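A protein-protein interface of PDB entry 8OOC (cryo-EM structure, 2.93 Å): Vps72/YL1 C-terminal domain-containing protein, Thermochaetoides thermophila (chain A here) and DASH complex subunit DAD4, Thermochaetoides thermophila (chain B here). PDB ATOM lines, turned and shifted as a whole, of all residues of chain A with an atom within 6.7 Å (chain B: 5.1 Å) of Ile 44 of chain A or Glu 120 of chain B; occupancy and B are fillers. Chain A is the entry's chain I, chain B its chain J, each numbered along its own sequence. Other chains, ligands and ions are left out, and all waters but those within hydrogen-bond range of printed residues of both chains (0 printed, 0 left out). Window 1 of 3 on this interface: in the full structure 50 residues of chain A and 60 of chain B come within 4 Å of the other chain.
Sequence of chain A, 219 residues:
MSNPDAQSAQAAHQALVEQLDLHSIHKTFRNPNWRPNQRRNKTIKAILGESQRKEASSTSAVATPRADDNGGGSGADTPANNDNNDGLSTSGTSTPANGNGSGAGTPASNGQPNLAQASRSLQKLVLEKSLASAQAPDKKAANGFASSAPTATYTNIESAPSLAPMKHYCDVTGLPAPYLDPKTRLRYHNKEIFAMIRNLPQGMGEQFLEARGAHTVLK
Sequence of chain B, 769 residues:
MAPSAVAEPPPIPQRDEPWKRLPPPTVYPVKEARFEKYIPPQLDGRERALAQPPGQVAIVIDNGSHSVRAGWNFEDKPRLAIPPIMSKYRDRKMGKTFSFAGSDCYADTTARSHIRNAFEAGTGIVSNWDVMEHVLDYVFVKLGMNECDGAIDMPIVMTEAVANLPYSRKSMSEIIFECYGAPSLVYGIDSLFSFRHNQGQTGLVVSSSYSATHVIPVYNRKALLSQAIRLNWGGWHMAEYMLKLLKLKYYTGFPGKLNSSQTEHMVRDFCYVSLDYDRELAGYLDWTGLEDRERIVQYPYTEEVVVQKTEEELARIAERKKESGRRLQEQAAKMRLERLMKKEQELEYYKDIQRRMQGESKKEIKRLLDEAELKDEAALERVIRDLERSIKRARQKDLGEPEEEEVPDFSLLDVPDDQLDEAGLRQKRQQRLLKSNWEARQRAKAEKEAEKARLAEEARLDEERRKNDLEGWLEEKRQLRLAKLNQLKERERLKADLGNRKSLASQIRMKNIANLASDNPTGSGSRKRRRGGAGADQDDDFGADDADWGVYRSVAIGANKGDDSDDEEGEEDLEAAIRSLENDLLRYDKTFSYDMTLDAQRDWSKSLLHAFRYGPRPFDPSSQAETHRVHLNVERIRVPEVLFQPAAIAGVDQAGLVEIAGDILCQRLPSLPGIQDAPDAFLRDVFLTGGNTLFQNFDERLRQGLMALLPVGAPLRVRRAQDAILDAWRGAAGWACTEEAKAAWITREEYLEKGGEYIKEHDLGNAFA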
ATOM      1  N   LYS A  42      15.441  -5.514 -27.884  1.00  0.00           N
ATOM      2  CA  LYS A  42      14.314  -4.752 -27.360  1.00  0.00           C
ATOM      3  C   LYS A  42      13.531  -5.597 -26.361  1.00  0.00           C
ATOM      4  O   LYS A  42      13.404  -6.814 -26.527  1.00  0.00           O
ATOM      5  CB  LYS A  42      13.383  -4.256 -28.472  1.00  0.00           C
ATOM      6  CG  LYS A  42      14.003  -3.189 -29.355  1.00  0.00           C
ATOM      7  CD  LYS A  42      13.003  -2.651 -30.361  1.00  0.00           C
ATOM      8  CE  LYS A  42      12.629  -3.704 -31.380  1.00  0.00           C
ATOM      9  NZ  LYS A  42      11.855  -3.135 -32.515  1.00  0.00           N
ATOM     10  N   THR A  43      13.010  -4.943 -25.324  1.00  0.00           N
ATOM     11  CA  THR A  43      12.167  -5.609 -24.341  1.00  0.00           C
ATOM     12  C   THR A  43      10.785  -5.922 -24.914  1.00  0.00           C
ATOM     13  O   THR A  43      10.337  -5.333 -25.902  1.00  0.00           O
ATOM     14  CB  THR A  43      12.023  -4.751 -23.085  1.00  0.00           C
ATOM     15  OG1 THR A  43      11.332  -3.538 -23.408  1.00  0.00           O
ATOM     16  CG2 THR A  43      13.389  -4.416 -22.510  1.00  0.00           C
ATOM     17  N   ILE A  44      10.112  -6.880 -24.269  1.00  0.00           N
ATOM     18  CA  ILE A  44       8.757  -7.272 -24.657  1.00  0.00           C
ATOM     19  C   ILE A  44       7.797  -6.089 -24.598  1.00  0.00           C
ATOM     20  O   ILE A  44       6.917  -5.942 -25.455  1.00  0.00           O
ATOM     21  CB  ILE A  44       8.270  -8.431 -23.767  1.00  0.00           C
ATOM     22  CG1 ILE A  44       9.179  -9.649 -23.931  1.00  0.00           C
ATOM     23  CG2 ILE A  44       6.830  -8.795 -24.096  1.00  0.00           C
ATOM     24  CD1 ILE A  44       9.136 -10.253 -25.306  1.00  0.00           C
ATOM     25  N   LYS A  45       7.945  -5.229 -23.588  1.00  0.00           N
ATOM     26  CA  LYS A  45       7.153  -4.002 -23.533  1.00  0.00           C
ATOM     27  C   LYS A  45       7.392  -3.129 -24.759  1.00  0.00           C
ATOM     28  O   LYS A  45       6.444  -2.623 -25.371  1.00  0.00           O
ATOM     29  CB  LYS A  45       7.464  -3.231 -22.250  1.00  0.00           C
ATOM     30  CG  LYS A  45       6.632  -1.970 -22.084  1.00  0.00           C
ATOM     31  CD  LYS A  45       6.963  -1.246 -20.792  1.00  0.00           C
ATOM     32  CE  LYS A  45       6.183   0.053 -20.680  1.00  0.00           C
ATOM     33  NZ  LYS A  45       6.508   0.798 -19.434  1.00  0.00           N
ATOM     34  N   ALA A  46       8.660  -2.929 -25.121  1.00  0.00           N
ATOM     35  CA  ALA A  46       8.992  -2.142 -26.305  1.00  0.00           C
ATOM     36  C   ALA A  46       8.412  -2.761 -27.574  1.00  0.00           C
ATOM     37  O   ALA A  46       7.834  -2.059 -28.411  1.00  0.00           O
ATOM     38  CB  ALA A  46      10.509  -1.994 -26.422  1.00  0.00           C
ATOM     39  N   ILE A  47       8.562  -4.079 -27.736  1.00  0.00           N
ATOM     40  CA  ILE A  47       8.037  -4.754 -28.921  1.00  0.00           C
ATOM     41  C   ILE A  47       6.520  -4.608 -29.004  1.00  0.00           C
ATOM     42  O   ILE A  47       5.969  -4.295 -30.066  1.00  0.00           O
ATOM     43  CB  ILE A  47       8.458  -6.233 -28.925  1.00  0.00           C
ATOM     44  CG1 ILE A  47       9.978  -6.352 -29.034  1.00  0.00           C
ATOM     45  CG2 ILE A  47       7.787  -6.973 -30.068  1.00  0.00           C
ATOM     46  CD1 ILE A  47      10.520  -7.684 -28.570  1.00  0.00           C
ATOM     47  N   LEU A  48       5.821  -4.836 -27.890  1.00  0.00           N
ATOM     48  CA  LEU A  48       4.371  -4.663 -27.892  1.00  0.00           C
ATOM     49  C   LEU A  48       3.980  -3.216 -28.173  1.00  0.00           C
ATOM     50  O   LEU A  48       3.019  -2.958 -28.907  1.00  0.00           O
ATOM     51  CB  LEU A  48       3.781  -5.129 -26.561  1.00  0.00           C
ATOM     52  CG  LEU A  48       3.787  -6.637 -26.312  1.00  0.00           C
ATOM     53  CD1 LEU A  48       3.419  -6.943 -24.870  1.00  0.00           C
ATOM     54  CD2 LEU A  48       2.839  -7.337 -27.270  1.00  0.00           C
ATOM     55  N   GLY A  49       4.706  -2.262 -27.593  1.00  0.00           N
ATOM     56  CA  GLY A  49       4.443  -0.862 -27.892  1.00  0.00           C
ATOM     57  C   GLY A  49       4.681  -0.519 -29.349  1.00  0.00           C
ATOM     58  O   GLY A  49       3.855   0.133 -29.993  1.00  0.00           O
ATOM     59  N   ASN A 156      -1.006 -13.673 -28.350  1.00  0.00           N
ATOM     60  CA  ASN A 156      -0.202 -13.278 -27.194  1.00  0.00           C
ATOM     61  C   ASN A 156      -0.988 -12.539 -26.110  1.00  0.00           C
ATOM     62  O   ASN A 156      -0.399 -12.079 -25.127  1.00  0.00           O
ATOM     63  CB  ASN A 156       0.987 -12.425 -27.654  1.00  0.00           C
ATOM     64  CG  ASN A 156       2.103 -12.376 -26.629  1.00  0.00           C
ATOM     65  OD1 ASN A 156       2.736 -13.389 -26.337  1.00  0.00           O
ATOM     66  ND2 ASN A 156       2.353 -11.192 -26.083  1.00  0.00           N
ATOM     67  N   ALA B 118      19.898 -15.026 -23.068  1.00  0.00           N
ATOM     68  CA  ALA B 118      19.204 -14.683 -24.305  1.00  0.00           C
ATOM     69  C   ALA B 118      17.751 -14.286 -24.074  1.00  0.00           C
ATOM     70  O   ALA B 118      17.226 -13.429 -24.794  1.00  0.00           O
ATOM     71  CB  ALA B 118      19.276 -15.854 -25.284  1.00  0.00           C
ATOM     72  N   PHE B 119      17.087 -14.886 -23.092  1.00  0.00           N
ATOM     73  CA  PHE B 119      15.667 -14.647 -22.882  1.00  0.00           C
ATOM     74  C   PHE B 119      15.445 -13.485 -21.925  1.00  0.00           C
ATOM     75  O   PHE B 119      16.258 -13.222 -21.035  1.00  0.00           O
ATOM     76  CB  PHE B 119      14.975 -15.902 -22.347  1.00  0.00           C
ATOM     77  CG  PHE B 119      14.910 -17.030 -23.336  1.00  0.00           C
ATOM     78  CD1 PHE B 119      15.966 -17.915 -23.478  1.00  0.00           C
ATOM     79  CD2 PHE B 119      13.784 -17.212 -24.119  1.00  0.00           C
ATOM     80  CE1 PHE B 119      15.901 -18.952 -24.390  1.00  0.00           C
ATOM     81  CE2 PHE B 119      13.712 -18.248 -25.028  1.00  0.00           C
ATOM     82  CZ  PHE B 119      14.772 -19.118 -25.163  1.00  0.00           C
ATOM     83  N   GLU B 120      14.328 -12.789 -22.119  1.00  0.00           N
ATOM     84  CA  GLU B 120      13.824 -11.892 -21.092  1.00  0.00           C
ATOM     85  C   GLU B 120      13.408 -12.684 -19.861  1.00  0.00           C
ATOM     86  O   GLU B 120      12.820 -13.765 -19.970  1.00  0.00           O
ATOM     87  CB  GLU B 120      12.646 -11.078 -21.625  1.00  0.00           C
ATOM     88  CG  GLU B 120      12.034 -10.139 -20.605  1.00  0.00           C
ATOM     89  CD  GLU B 120      11.255  -9.016 -21.248  1.00  0.00           C
ATOM     90  OE1 GLU B 120      11.774  -8.406 -22.207  1.00  0.00           O
ATOM     91  OE2 GLU B 120      10.125  -8.742 -20.794  1.00  0.00           O
ATOM     92  N   ALA B 121      13.737 -12.146 -18.687  1.00  0.00           N
ATOM     93  CA  ALA B 121      13.616 -12.892 -17.440  1.00  0.00           C
ATOM     94  C   ALA B 121      12.209 -13.442 -17.246  1.00  0.00           C
ATOM     95  O   ALA B 121      11.219 -12.713 -17.352  1.00  0.00           O
ATOM     96  CB  ALA B 121      13.997 -11.994 -16.261  1.00  0.00           C
ATOM     97  N   GLY B 122      12.133 -14.738 -16.960  1.00  0.00           N
ATOM     98  CA  GLY B 122      10.873 -15.425 -16.756  1.00  0.00           C
ATOM     99  C   GLY B 122       9.921 -15.477 -17.931  1.00  0.00           C
ATOM    100  O   GLY B 122       8.749 -15.825 -17.761  1.00  0.00           O
ATOM    101  N   THR B 123      10.398 -15.141 -19.124  1.00  0.00           N
ATOM    102  CA  THR B 123       9.526 -14.930 -20.266  1.00  0.00           C
ATOM    103  C   THR B 123       9.933 -15.868 -21.393  1.00  0.00           C
ATOM    104  O   THR B 123      11.109 -16.210 -21.544  1.00  0.00           O
ATOM    105  CB  THR B 123       9.576 -13.467 -20.736  1.00  0.00           C
ATOM    106  OG1 THR B 123       9.330 -12.603 -19.620  1.00  0.00           O
ATOM    107  CG2 THR B 123       8.518 -13.195 -21.791  1.00  0.00           C
ATOM    108  N   ILE B 125      10.136 -15.623 -24.564  1.00  0.00           N
ATOM    109  CA  ILE B 125      10.467 -15.010 -25.841  1.00  0.00           C
ATOM    110  C   ILE B 125      11.908 -14.517 -25.796  1.00  0.00           C
ATOM    111  O   ILE B 125      12.326 -13.892 -24.815  1.00  0.00           O
ATOM    112  CB  ILE B 125       9.492 -13.864 -26.163  1.00  0.00           C
ATOM    113  CG1 ILE B 125       8.094 -14.436 -26.402  1.00  0.00           C
ATOM    114  CG2 ILE B 125       9.960 -13.082 -27.368  1.00  0.00           C
ATOM    115  CD1 ILE B 125       7.054 -13.399 -26.712  1.00  0.00           C
ATOM    116  N   VAL B 126      12.657 -14.795 -26.865  1.00  0.00           N
ATOM    117  CA  VAL B 126      14.044 -14.357 -26.974  1.00  0.00           C
ATOM    118  C   VAL B 126      14.104 -12.842 -27.131  1.00  0.00           C
ATOM    119  O   VAL B 126      13.269 -12.235 -27.816  1.00  0.00           O
ATOM    120  CB  VAL B 126      14.731 -15.070 -28.151  1.00  0.00           C
ATOM    121  CG1 VAL B 126      16.163 -14.585 -28.316  1.00  0.00           C
ATOM    122  CG2 VAL B 126      14.689 -16.575 -27.959  1.00  0.00           C
ATOM    123  N   SER B 127      15.101 -12.221 -26.493  1.00  0.00           N
ATOM    124  CA  SER B 127      15.199 -10.764 -26.463  1.00  0.00           C
ATOM    125  C   SER B 127      16.619 -10.223 -26.594  1.00  0.00           C
ATOM    126  O   SER B 127      16.787  -9.151 -27.184  1.00  0.00           O
ATOM    127  CB  SER B 127      14.579 -10.212 -25.173  1.00  0.00           C
ATOM    128  OG  SER B 127      14.851  -8.830 -25.030  1.00  0.00           O
ATOM    129  N   LEU B 165       6.194 -13.559 -30.651  1.00  0.00           N
ATOM    130  CA  LEU B 165       5.996 -12.229 -31.208  1.00  0.00           C
ATOM    131  C   LEU B 165       6.568 -12.147 -32.623  1.00  0.00           C
ATOM    132  O   LEU B 165       7.613 -12.741 -32.905  1.00  0.00           O
ATOM    133  CB  LEU B 165       6.642 -11.161 -30.326  1.00  0.00           C
ATOM    134  CG  LEU B 165       5.973 -10.856 -28.987  1.00  0.00           C
ATOM    135  CD1 LEU B 165       6.884 -10.004 -28.125  1.00  0.00           C
ATOM    136  CD2 LEU B 165       4.633 -10.166 -29.190  1.00  0.00           C
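The backbone carbonyl oxygen of Lys 42 of chain A sits at hydrogen-bond distance from the side-chain hydroxyl of Ser 127 of chain B, 2.9 Å away.
N of Ile 44 of chain A lies within hydrogen-bond range of OE1 of Glu 120 of chain B (3.1 Å).
OG1 of Thr 43 of chain A sits at hydrogen-bond distance from N of Ala 46 of chain A, 3.2 Å away.
N of Ser 127 of chain B lies within hydrogen-bond range of O of Ala 118 of chain B, 3.0 Å away.
Among the printed residues, pairs that only touch across the chains: Thr 43 of chain A with Glu 120 of chain B (3.5 Å), Ile 44 of chain A with Ile 125 of chain B (3.6 Å), Ile 44 of chain A with Leu 165 of chain B (3.6 Å), Ile 47 of chain A with Leu 165 of chain B (3.7 Å), Leu 48 of chain A with Leu 165 of chain B (3.9 Å) and Asn 156 of chain A with Leu 165 of chain B (3.99 Å).
Ile 44 of chain A touches just these residues of chain B: Glu 120 (3.1 Å), Ile 125 (3.6 Å) and Leu 165 (3.6 Å).
Glu 120 of chain B touches just these residues of chain A: Thr 43 (3.5 Å) and Ile 44 (3.1 Å).
Of the printed residues of chain B, Lys 42 of chain A touches Ser 127.
Of the printed residues of chain B, Asn 156 of chain A touches Leu 165 (3.99 Å).
Printed residues of chain B within 4 Å of Ile 47 of chain A: Leu 165 (3.7 Å).
Printed residues of chain A within 4 Å of Ile 125 of chain B: Ile 44.
Printed residues of chain B within 4 Å of Leu 48 of chain A: Leu 165.
Lys 45 of chain A touches none of the printed residues of chain B.
Gly 122 of chain B touches none of the printed residues of chain A.
The nearest residue of chain A that does not touch Glu 120 of chain B is Lys 42 of chain A (4.9 Å).
The nearest printed residue of chain A that does not touch Ile 125 of chain B is Asn 156 of chain A (4.3 Å).
Hydrophobic or aromatic side chains of chain A that line the printed part of chain B: Ile 44, Ile 47 and Leu 48.
Hydrophobic or aromatic side chains of chain B that line the printed part of chain A: Ile 125 and Leu 165.
Among the printed residues, 8 pairs touch across the chains.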
